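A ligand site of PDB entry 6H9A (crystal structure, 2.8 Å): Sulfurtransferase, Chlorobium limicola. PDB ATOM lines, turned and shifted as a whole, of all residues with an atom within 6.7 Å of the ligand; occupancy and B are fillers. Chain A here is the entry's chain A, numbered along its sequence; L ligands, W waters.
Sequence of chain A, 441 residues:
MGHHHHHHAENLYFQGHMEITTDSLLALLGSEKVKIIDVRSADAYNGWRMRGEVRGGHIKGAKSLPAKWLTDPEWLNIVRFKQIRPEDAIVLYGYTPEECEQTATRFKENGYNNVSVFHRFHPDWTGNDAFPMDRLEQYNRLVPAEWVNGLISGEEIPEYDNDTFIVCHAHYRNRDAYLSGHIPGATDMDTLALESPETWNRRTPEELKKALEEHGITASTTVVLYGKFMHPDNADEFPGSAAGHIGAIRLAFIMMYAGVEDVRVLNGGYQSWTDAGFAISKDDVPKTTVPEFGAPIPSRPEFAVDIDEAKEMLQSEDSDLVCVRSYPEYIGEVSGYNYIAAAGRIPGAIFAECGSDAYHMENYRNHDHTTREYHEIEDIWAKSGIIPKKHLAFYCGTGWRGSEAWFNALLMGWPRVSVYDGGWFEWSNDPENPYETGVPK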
ATOM      1  N   TYR A 172      12.818   9.872  29.149  1.00  0.00           N
ATOM      2  CA  TYR A 172      13.204   8.471  29.347  1.00  0.00           C
ATOM      3  C   TYR A 172      14.577   8.258  28.729  1.00  0.00           C
ATOM      4  O   TYR A 172      14.708   8.206  27.501  1.00  0.00           O
ATOM      5  CB  TYR A 172      12.170   7.535  28.722  1.00  0.00           C
ATOM      6  CG  TYR A 172      12.599   6.088  28.678  1.00  0.00           C
ATOM      7  CD1 TYR A 172      12.966   5.425  29.845  1.00  0.00           C
ATOM      8  CD2 TYR A 172      12.616   5.384  27.489  1.00  0.00           C
ATOM      9  CE1 TYR A 172      13.357   4.102  29.812  1.00  0.00           C
ATOM     10  CE2 TYR A 172      13.008   4.061  27.447  1.00  0.00           C
ATOM     11  CZ  TYR A 172      13.369   3.417  28.613  1.00  0.00           C
ATOM     12  OH  TYR A 172      13.757   2.103  28.571  1.00  0.00           O
ATOM     13  N   THR A 191      12.460   9.141  33.746  1.00  0.00           N
ATOM     14  CA  THR A 191      11.380   8.305  34.245  1.00  0.00           C
ATOM     15  C   THR A 191      11.898   7.076  34.986  1.00  0.00           C
ATOM     16  O   THR A 191      11.185   6.536  35.825  1.00  0.00           O
ATOM     17  CB  THR A 191      10.469   7.872  33.091  1.00  0.00           C
ATOM     18  OG1 THR A 191      11.258   7.402  31.992  1.00  0.00           O
ATOM     19  CG2 THR A 191       9.599   9.033  32.627  1.00  0.00           C
ATOM     20  N   LEU A 192      13.124   6.647  34.697  1.00  0.00           N
ATOM     21  CA  LEU A 192      13.713   5.523  35.404  1.00  0.00           C
ATOM     22  C   LEU A 192      13.942   5.808  36.883  1.00  0.00           C
ATOM     23  O   LEU A 192      14.213   4.879  37.645  1.00  0.00           O
ATOM     24  CB  LEU A 192      15.028   5.115  34.740  1.00  0.00           C
ATOM     25  CG  LEU A 192      14.889   4.417  33.389  1.00  0.00           C
ATOM     26  CD1 LEU A 192      16.214   4.410  32.652  1.00  0.00           C
ATOM     27  CD2 LEU A 192      14.380   2.995  33.581  1.00  0.00           C
ATOM     28  N   GLU A 195      10.304   4.530  38.142  1.00  0.00           N
ATOM     29  CA  GLU A 195       9.890   3.184  37.769  1.00  0.00           C
ATOM     30  C   GLU A 195      11.117   2.338  37.472  1.00  0.00           C
ATOM     31  O   GLU A 195      12.089   2.828  36.890  1.00  0.00           O
ATOM     32  CB  GLU A 195       8.934   3.198  36.565  1.00  0.00           C
ATOM     33  CG  GLU A 195       9.459   3.914  35.344  1.00  0.00           C
ATOM     34  CD  GLU A 195       8.511   3.836  34.160  1.00  0.00           C
ATOM     35  OE1 GLU A 195       8.903   4.217  33.047  1.00  0.00           O
ATOM     36  OE2 GLU A 195       7.363   3.379  34.359  1.00  0.00           O
ATOM     37  N   TRP A 200       9.099  -2.688  35.365  1.00  0.00           N
ATOM     38  CA  TRP A 200       8.450  -1.572  34.670  1.00  0.00           C
ATOM     39  C   TRP A 200       7.241  -1.049  35.429  1.00  0.00           C
ATOM     40  O   TRP A 200       6.358  -0.413  34.849  1.00  0.00           O
ATOM     41  CB  TRP A 200       8.062  -1.948  33.230  1.00  0.00           C
ATOM     42  CG  TRP A 200       9.247  -2.006  32.310  1.00  0.00           C
ATOM     43  CD1 TRP A 200       9.577  -3.026  31.468  1.00  0.00           C
ATOM     44  CD2 TRP A 200      10.259  -0.995  32.134  1.00  0.00           C
ATOM     45  NE1 TRP A 200      10.726  -2.721  30.778  1.00  0.00           N
ATOM     46  CE2 TRP A 200      11.174  -1.481  31.170  1.00  0.00           C
ATOM     47  CE3 TRP A 200      10.490   0.261  32.697  1.00  0.00           C
ATOM     48  CZ2 TRP A 200      12.281  -0.752  30.761  1.00  0.00           C
ATOM     49  CZ3 TRP A 200      11.597   0.989  32.288  1.00  0.00           C
ATOM     50  CH2 TRP A 200      12.480   0.474  31.326  1.00  0.00           C
ATOM     51  N   PHE A 238      14.975   3.100  21.506  1.00  0.00           N
ATOM     52  CA  PHE A 238      14.198   3.573  22.644  1.00  0.00           C
ATOM     53  C   PHE A 238      13.226   4.651  22.156  1.00  0.00           C
ATOM     54  O   PHE A 238      13.496   5.851  22.307  1.00  0.00           O
ATOM     55  CB  PHE A 238      15.100   4.098  23.758  1.00  0.00           C
ATOM     56  CG  PHE A 238      16.011   3.063  24.339  1.00  0.00           C
ATOM     57  CD1 PHE A 238      15.530   2.113  25.228  1.00  0.00           C
ATOM     58  CD2 PHE A 238      17.355   3.026  24.002  1.00  0.00           C
ATOM     59  CE1 PHE A 238      16.371   1.161  25.762  1.00  0.00           C
ATOM     60  CE2 PHE A 238      18.205   2.078  24.535  1.00  0.00           C
ATOM     61  CZ  PHE A 238      17.709   1.144  25.415  1.00  0.00           C
ATOM     62  N   PRO A 239      12.091   4.259  21.574  1.00  0.00           N
ATOM     63  CA  PRO A 239      11.122   5.265  21.116  1.00  0.00           C
ATOM     64  C   PRO A 239      10.531   6.088  22.243  1.00  0.00           C
ATOM     65  O   PRO A 239      10.053   7.199  21.981  1.00  0.00           O
ATOM     66  CB  PRO A 239      10.055   4.424  20.403  1.00  0.00           C
ATOM     67  CG  PRO A 239      10.716   3.102  20.116  1.00  0.00           C
ATOM     68  CD  PRO A 239      11.666   2.889  21.251  1.00  0.00           C
ATOM     69  N   GLY A 240      10.541   5.576  23.477  1.00  0.00           N
ATOM     70  CA  GLY A 240      10.014   6.324  24.600  1.00  0.00           C
ATOM     71  C   GLY A 240      10.797   7.584  24.906  1.00  0.00           C
ATOM     72  O   GLY A 240      10.261   8.491  25.558  1.00  0.00           O
ATOM     73  N   SER A 241      12.047   7.667  24.463  1.00  0.00           N
ATOM     74  CA  SER A 241      12.836   8.888  24.657  1.00  0.00           C
ATOM     75  C   SER A 241      12.226  10.079  23.931  1.00  0.00           C
ATOM     76  O   SER A 241      12.554  11.221  24.269  1.00  0.00           O
ATOM     77  CB  SER A 241      14.273   8.661  24.177  1.00  0.00           C
ATOM     78  OG  SER A 241      14.924   7.691  24.980  1.00  0.00           O
ATOM     79  N   ALA A 243       8.677  10.173  23.476  1.00  0.00           N
ATOM     80  CA  ALA A 243       7.313  10.306  23.994  1.00  0.00           C
ATOM     81  C   ALA A 243       7.338  11.000  25.351  1.00  0.00           C
ATOM     82  O   ALA A 243       6.916  10.464  26.376  1.00  0.00           O
ATOM     83  CB  ALA A 243       6.658   8.935  24.083  1.00  0.00           C
ATOM     84  N   ILE A 246       3.865  11.751  27.402  1.00  0.00           N
ATOM     85  CA  ILE A 246       3.272  10.571  28.018  1.00  0.00           C
ATOM     86  C   ILE A 246       3.996  10.235  29.316  1.00  0.00           C
ATOM     87  O   ILE A 246       3.361   9.916  30.340  1.00  0.00           O
ATOM     88  CB  ILE A 246       3.285   9.372  27.053  1.00  0.00           C
ATOM     89  CG1 ILE A 246       2.724   9.779  25.687  1.00  0.00           C
ATOM     90  CG2 ILE A 246       2.485   8.213  27.619  1.00  0.00           C
ATOM     91  CD1 ILE A 246       2.589   8.619  24.718  1.00  0.00           C
ATOM     92  N   GLY A 247       5.329  10.327  29.309  1.00  0.00           N
ATOM     93  CA  GLY A 247       6.082  10.085  30.524  1.00  0.00           C
ATOM     94  C   GLY A 247       5.824  11.113  31.603  1.00  0.00           C
ATOM     95  O   GLY A 247       5.868  10.791  32.794  1.00  0.00           O
ATOM     96  N   GLY A 336       3.921  -4.858  20.494  1.00  0.00           N
ATOM     97  CA  GLY A 336       3.890  -3.426  20.649  1.00  0.00           C
ATOM     98  C   GLY A 336       5.172  -2.810  21.153  1.00  0.00           C
ATOM     99  O   GLY A 336       5.310  -1.587  21.120  1.00  0.00           O
ATOM    100  N   TYR A 337       6.118  -3.635  21.620  1.00  0.00           N
ATOM    101  CA  TYR A 337       7.377  -3.142  22.166  1.00  0.00           C
ATOM    102  C   TYR A 337       8.521  -4.022  21.683  1.00  0.00           C
ATOM    103  O   TYR A 337       8.325  -5.208  21.408  1.00  0.00           O
ATOM    104  CB  TYR A 337       7.359  -3.100  23.699  1.00  0.00           C
ATOM    105  CG  TYR A 337       6.212  -2.327  24.302  1.00  0.00           C
ATOM    106  CD1 TYR A 337       4.964  -2.907  24.478  1.00  0.00           C
ATOM    107  CD2 TYR A 337       6.384  -1.003  24.708  1.00  0.00           C
ATOM    108  CE1 TYR A 337       3.917  -2.197  25.027  1.00  0.00           C
ATOM    109  CE2 TYR A 337       5.346  -0.290  25.256  1.00  0.00           C
ATOM    110  CZ  TYR A 337       4.113  -0.887  25.421  1.00  0.00           C
ATOM    111  OH  TYR A 337       3.066  -0.176  25.970  1.00  0.00           O
ATOM    112  N   ASN A 338       9.707  -3.430  21.591  1.00  0.00           N
ATOM    113  CA  ASN A 338      10.913  -4.178  21.264  1.00  0.00           C
ATOM    114  C   ASN A 338      11.552  -4.832  22.477  1.00  0.00           C
ATOM    115  O   ASN A 338      12.634  -5.411  22.366  1.00  0.00           O
ATOM    116  CB  ASN A 338      11.928  -3.265  20.558  1.00  0.00           C
ATOM    117  CG  ASN A 338      12.473  -2.189  21.467  1.00  0.00           C
ATOM    118  OD1 ASN A 338      11.899  -1.883  22.505  1.00  0.00           O
ATOM    119  ND2 ASN A 338      13.602  -1.600  21.058  1.00  0.00           N
ATOM    120  N   TYR A 339      10.896  -4.751  23.641  1.00  0.00           N
ATOM    121  CA  TYR A 339      11.360  -5.416  24.853  1.00  0.00           C
ATOM    122  C   TYR A 339      10.276  -6.286  25.482  1.00  0.00           C
ATOM    123  O   TYR A 339      10.461  -6.774  26.597  1.00  0.00           O
ATOM    124  CB  TYR A 339      11.865  -4.394  25.874  1.00  0.00           C
ATOM    125  CG  TYR A 339      10.810  -3.403  26.312  1.00  0.00           C
ATOM    126  CD1 TYR A 339      10.549  -2.262  25.558  1.00  0.00           C
ATOM    127  CD2 TYR A 339      10.081  -3.595  27.481  1.00  0.00           C
ATOM    128  CE1 TYR A 339       9.590  -1.356  25.942  1.00  0.00           C
ATOM    129  CE2 TYR A 339       9.123  -2.689  27.874  1.00  0.00           C
ATOM    130  CZ  TYR A 339       8.879  -1.574  27.110  1.00  0.00           C
ATOM    131  OH  TYR A 339       7.922  -0.667  27.503  1.00  0.00           O
ATOM    132  N   ALA A 358       2.308   2.150  20.139  1.00  0.00           N
ATOM    133  CA  ALA A 358       2.433   2.257  21.584  1.00  0.00           C
ATOM    134  C   ALA A 358       3.013   3.590  22.039  1.00  0.00           C
ATOM    135  O   ALA A 358       3.098   3.823  23.245  1.00  0.00           O
ATOM    136  CB  ALA A 358       3.302   1.116  22.127  1.00  0.00           C
ATOM    137  N   TYR A 359       3.411   4.463  21.114  1.00  0.00           N
ATOM    138  CA  TYR A 359       4.060   5.723  21.475  1.00  0.00           C
ATOM    139  C   TYR A 359       3.278   6.933  20.968  1.00  0.00           C
ATOM    140  O   TYR A 359       3.826   8.041  20.895  1.00  0.00           O
ATOM    141  CB  TYR A 359       5.491   5.747  20.943  1.00  0.00           C
ATOM    142  CG  TYR A 359       6.330   4.596  21.458  1.00  0.00           C
ATOM    143  CD1 TYR A 359       7.037   4.705  22.644  1.00  0.00           C
ATOM    144  CD2 TYR A 359       6.407   3.403  20.760  1.00  0.00           C
ATOM    145  CE1 TYR A 359       7.801   3.658  23.122  1.00  0.00           C
ATOM    146  CE2 TYR A 359       7.172   2.346  21.227  1.00  0.00           C
ATOM    147  CZ  TYR A 359       7.862   2.481  22.414  1.00  0.00           C
ATOM    148  OH  TYR A 359       8.624   1.433  22.882  1.00  0.00           O
ATOM    149  N   HIS A 360       2.006   6.758  20.631  1.00  0.00           N
ATOM    150  CA  HIS A 360       1.165   7.855  20.167  1.00  0.00           C
ATOM    151  C   HIS A 360      -0.220   7.730  20.787  1.00  0.00           C
ATOM    152  O   HIS A 360      -0.730   6.621  20.968  1.00  0.00           O
ATOM    153  CB  HIS A 360       1.054   7.858  18.630  1.00  0.00           C
ATOM    154  CG  HIS A 360       2.351   8.124  17.934  1.00  0.00           C
ATOM    155  ND1 HIS A 360       3.336   7.171  17.809  1.00  0.00           N
ATOM    156  CD2 HIS A 360       2.818   9.234  17.324  1.00  0.00           C
ATOM    157  CE1 HIS A 360       4.359   7.688  17.155  1.00  0.00           C
ATOM    158  NE2 HIS A 360       4.075   8.943  16.843  1.00  0.00           N
ATOM    159  N   CYS A 396      -1.840  -0.645  29.981  1.00  0.00           N
ATOM    160  CA  CYS A 396      -1.352  -0.859  28.626  1.00  0.00           C
ATOM    161  C   CYS A 396      -0.222  -1.885  28.645  1.00  0.00           C
ATOM    162  O   CYS A 396      -0.305  -2.900  29.345  1.00  0.00           O
ATOM    163  CB  CYS A 396      -0.897   0.457  27.986  1.00  0.00           C
ATOM    164  SG  CYS A 396       0.581   1.192  28.720  1.00  0.00           S
ATOM    165  N   GLY A 397       0.851  -1.613  27.900  1.00  0.00           N
ATOM    166  CA  GLY A 397       2.009  -2.484  27.947  1.00  0.00           C
ATOM    167  C   GLY A 397       2.675  -2.483  29.305  1.00  0.00           C
ATOM    168  O   GLY A 397       2.730  -3.508  29.989  1.00  0.00           O
ATOM    169  N   THR A 398       3.188  -1.317  29.714  1.00  0.00           N
ATOM    170  CA  THR A 398       3.826  -1.167  31.004  1.00  0.00           C
ATOM    171  C   THR A 398       3.162  -0.145  31.912  1.00  0.00           C
ATOM    172  O   THR A 398       3.361  -0.212  33.135  1.00  0.00           O
ATOM    173  CB  THR A 398       5.310  -0.776  30.838  1.00  0.00           C
ATOM    174  OG1 THR A 398       5.402   0.493  30.176  1.00  0.00           O
ATOM    175  CG2 THR A 398       6.040  -1.831  30.026  1.00  0.00           C
ATOM    176  N   GLY A 399       2.387   0.796  31.376  1.00  0.00           N
ATOM    177  CA  GLY A 399       1.655   1.724  32.208  1.00  0.00           C
ATOM    178  C   GLY A 399       1.601   3.156  31.723  1.00  0.00           C
ATOM    179  O   GLY A 399       0.788   3.948  32.230  1.00  0.00           O
ATOM    180  N   TRP A 400       2.437   3.514  30.759  1.00  0.00           N
ATOM    181  CA  TRP A 400       2.483   4.892  30.279  1.00  0.00           C
ATOM    182  C   TRP A 400       1.173   5.305  29.641  1.00  0.00           C
ATOM    183  O   TRP A 400       0.544   6.301  30.038  1.00  0.00           O
ATOM    184  CB  TRP A 400       3.643   5.078  29.289  1.00  0.00           C
ATOM    185  CG  TRP A 400       4.967   5.307  29.943  1.00  0.00           C
ATOM    186  CD1 TRP A 400       5.424   4.724  31.095  1.00  0.00           C
ATOM    187  CD2 TRP A 400       5.994   6.189  29.497  1.00  0.00           C
ATOM    188  NE1 TRP A 400       6.689   5.190  31.380  1.00  0.00           N
ATOM    189  CE2 TRP A 400       7.066   6.089  30.415  1.00  0.00           C
ATOM    190  CE3 TRP A 400       6.139   7.039  28.394  1.00  0.00           C
ATOM    191  CZ2 TRP A 400       8.240   6.814  30.273  1.00  0.00           C
ATOM    192  CZ3 TRP A 400       7.303   7.761  28.252  1.00  0.00           C
ATOM    193  CH2 TRP A 400       8.351   7.642  29.192  1.00  0.00           C
ATOM    194  N   ARG A 401       0.723   4.551  28.626  1.00  0.00           N
ATOM    195  CA  ARG A 401      -0.524   4.888  27.945  1.00  0.00           C
ATOM    196  C   ARG A 401      -1.723   4.754  28.877  1.00  0.00           C
ATOM    197  O   ARG A 401      -2.677   5.531  28.770  1.00  0.00           O
ATOM    198  CB  ARG A 401      -0.706   4.009  26.717  1.00  0.00           C
ATOM    199  CG  ARG A 401       0.329   4.241  25.633  1.00  0.00           C
ATOM    200  CD  ARG A 401       0.178   3.245  24.505  1.00  0.00           C
ATOM    201  NE  ARG A 401       0.548   1.900  24.933  1.00  0.00           N
ATOM    202  CZ  ARG A 401       0.334   0.797  24.209  1.00  0.00           C
ATOM    203  NH1 ARG A 401      -0.248   0.893  23.016  1.00  0.00           N
ATOM    204  NH2 ARG A 401       0.697  -0.383  24.667  1.00  0.00           N
HETATM  205  C1  LIG L   1       8.673   1.585  30.038  1.00  0.00           C
HETATM  206  C2  LIG L   1       9.906   3.526  29.296  1.00  0.00           C
HETATM  207  C3  LIG L   1      10.424   1.330  28.380  1.00  0.00           C
HETATM  208  O1  LIG L   1       9.684   3.407  26.103  1.00  0.00           O
HETATM  209  O2  LIG L   1       8.612   1.539  25.515  1.00  0.00           O
HETATM  210  C4  LIG L   1       6.042   4.745  25.917  1.00  0.00           C
HETATM  211  C5  LIG L   1       7.416   3.732  27.907  1.00  0.00           C
HETATM  212  N1  LIG L   1       5.191   3.012  26.970  1.00  0.00           N
HETATM  213  N2  LIG L   1       4.829   4.434  25.328  1.00  0.00           N
HETATM  214  C6  LIG L   1       8.871   2.404  26.329  1.00  0.00           C
HETATM  215  C7  LIG L   1       6.273   3.854  26.952  1.00  0.00           C
HETATM  216  C8  LIG L   1       4.354   3.394  25.988  1.00  0.00           C
HETATM  217  C9  LIG L   1       8.235   2.458  27.712  1.00  0.00           C
HETATM  218  N3  LIG L   1       9.317   2.222  28.841  1.00  0.00           N
HETATM  219  O   HOH W   1       3.923   1.377  28.443  1.00  0.00           O
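Merely in contact with the ligand: Trp 400, Gly 240, Tyr 172, Thr 398, Tyr 337, Trp 200 and Glu 195. Hydrophobic or aromatic side chains that line the ligand: Tyr 172, Trp 200, Tyr 337, Tyr 339, Tyr 359 and Trp 400.
N of Trp 400 lies within hydrogen-bond range of SG of Cys 396. NE1 of Trp 400 lies within hydrogen-bond range of OE1 of Glu 195 (2.9 Å). The side-chain hydroxyl (OH) of Tyr 337 is in hydrogen-bond range of the guanidinium group (NH2) of Arg 401 (2.7 Å). OG of Ser 241 sits at hydrogen-bond distance from O of Tyr 172 (2.6 Å). The side-chain hydroxyl (OH) of Tyr 337 sits close to the backbone NH (N) of Gly 397. The backbone NH (N) of Thr 398 sits close to the side-chain sulfur (SG) of Cys 396, at 3.8 Å.
The side-chain hydroxyl (OH) of Tyr 339 lies within hydrogen-bond range of an oxygen (O2) of the ligand (3.0 Å). O of Ala 358 lies close to N2 of the ligand, at 2.8 Å. OH of Tyr 359 is in hydrogen-bond range of O2 of the ligand (2.6 Å).
Water W1 lies within hydrogen-bond range of OG1 of Thr 398 (2.4 Å), N1 of the ligand (2.5 Å), OH of Tyr 337 (3.0 Å), SG of Cys 396 (3.4 Å), N of Gly 399 (3.4 Å) and N of Trp 400 (3.5 Å).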
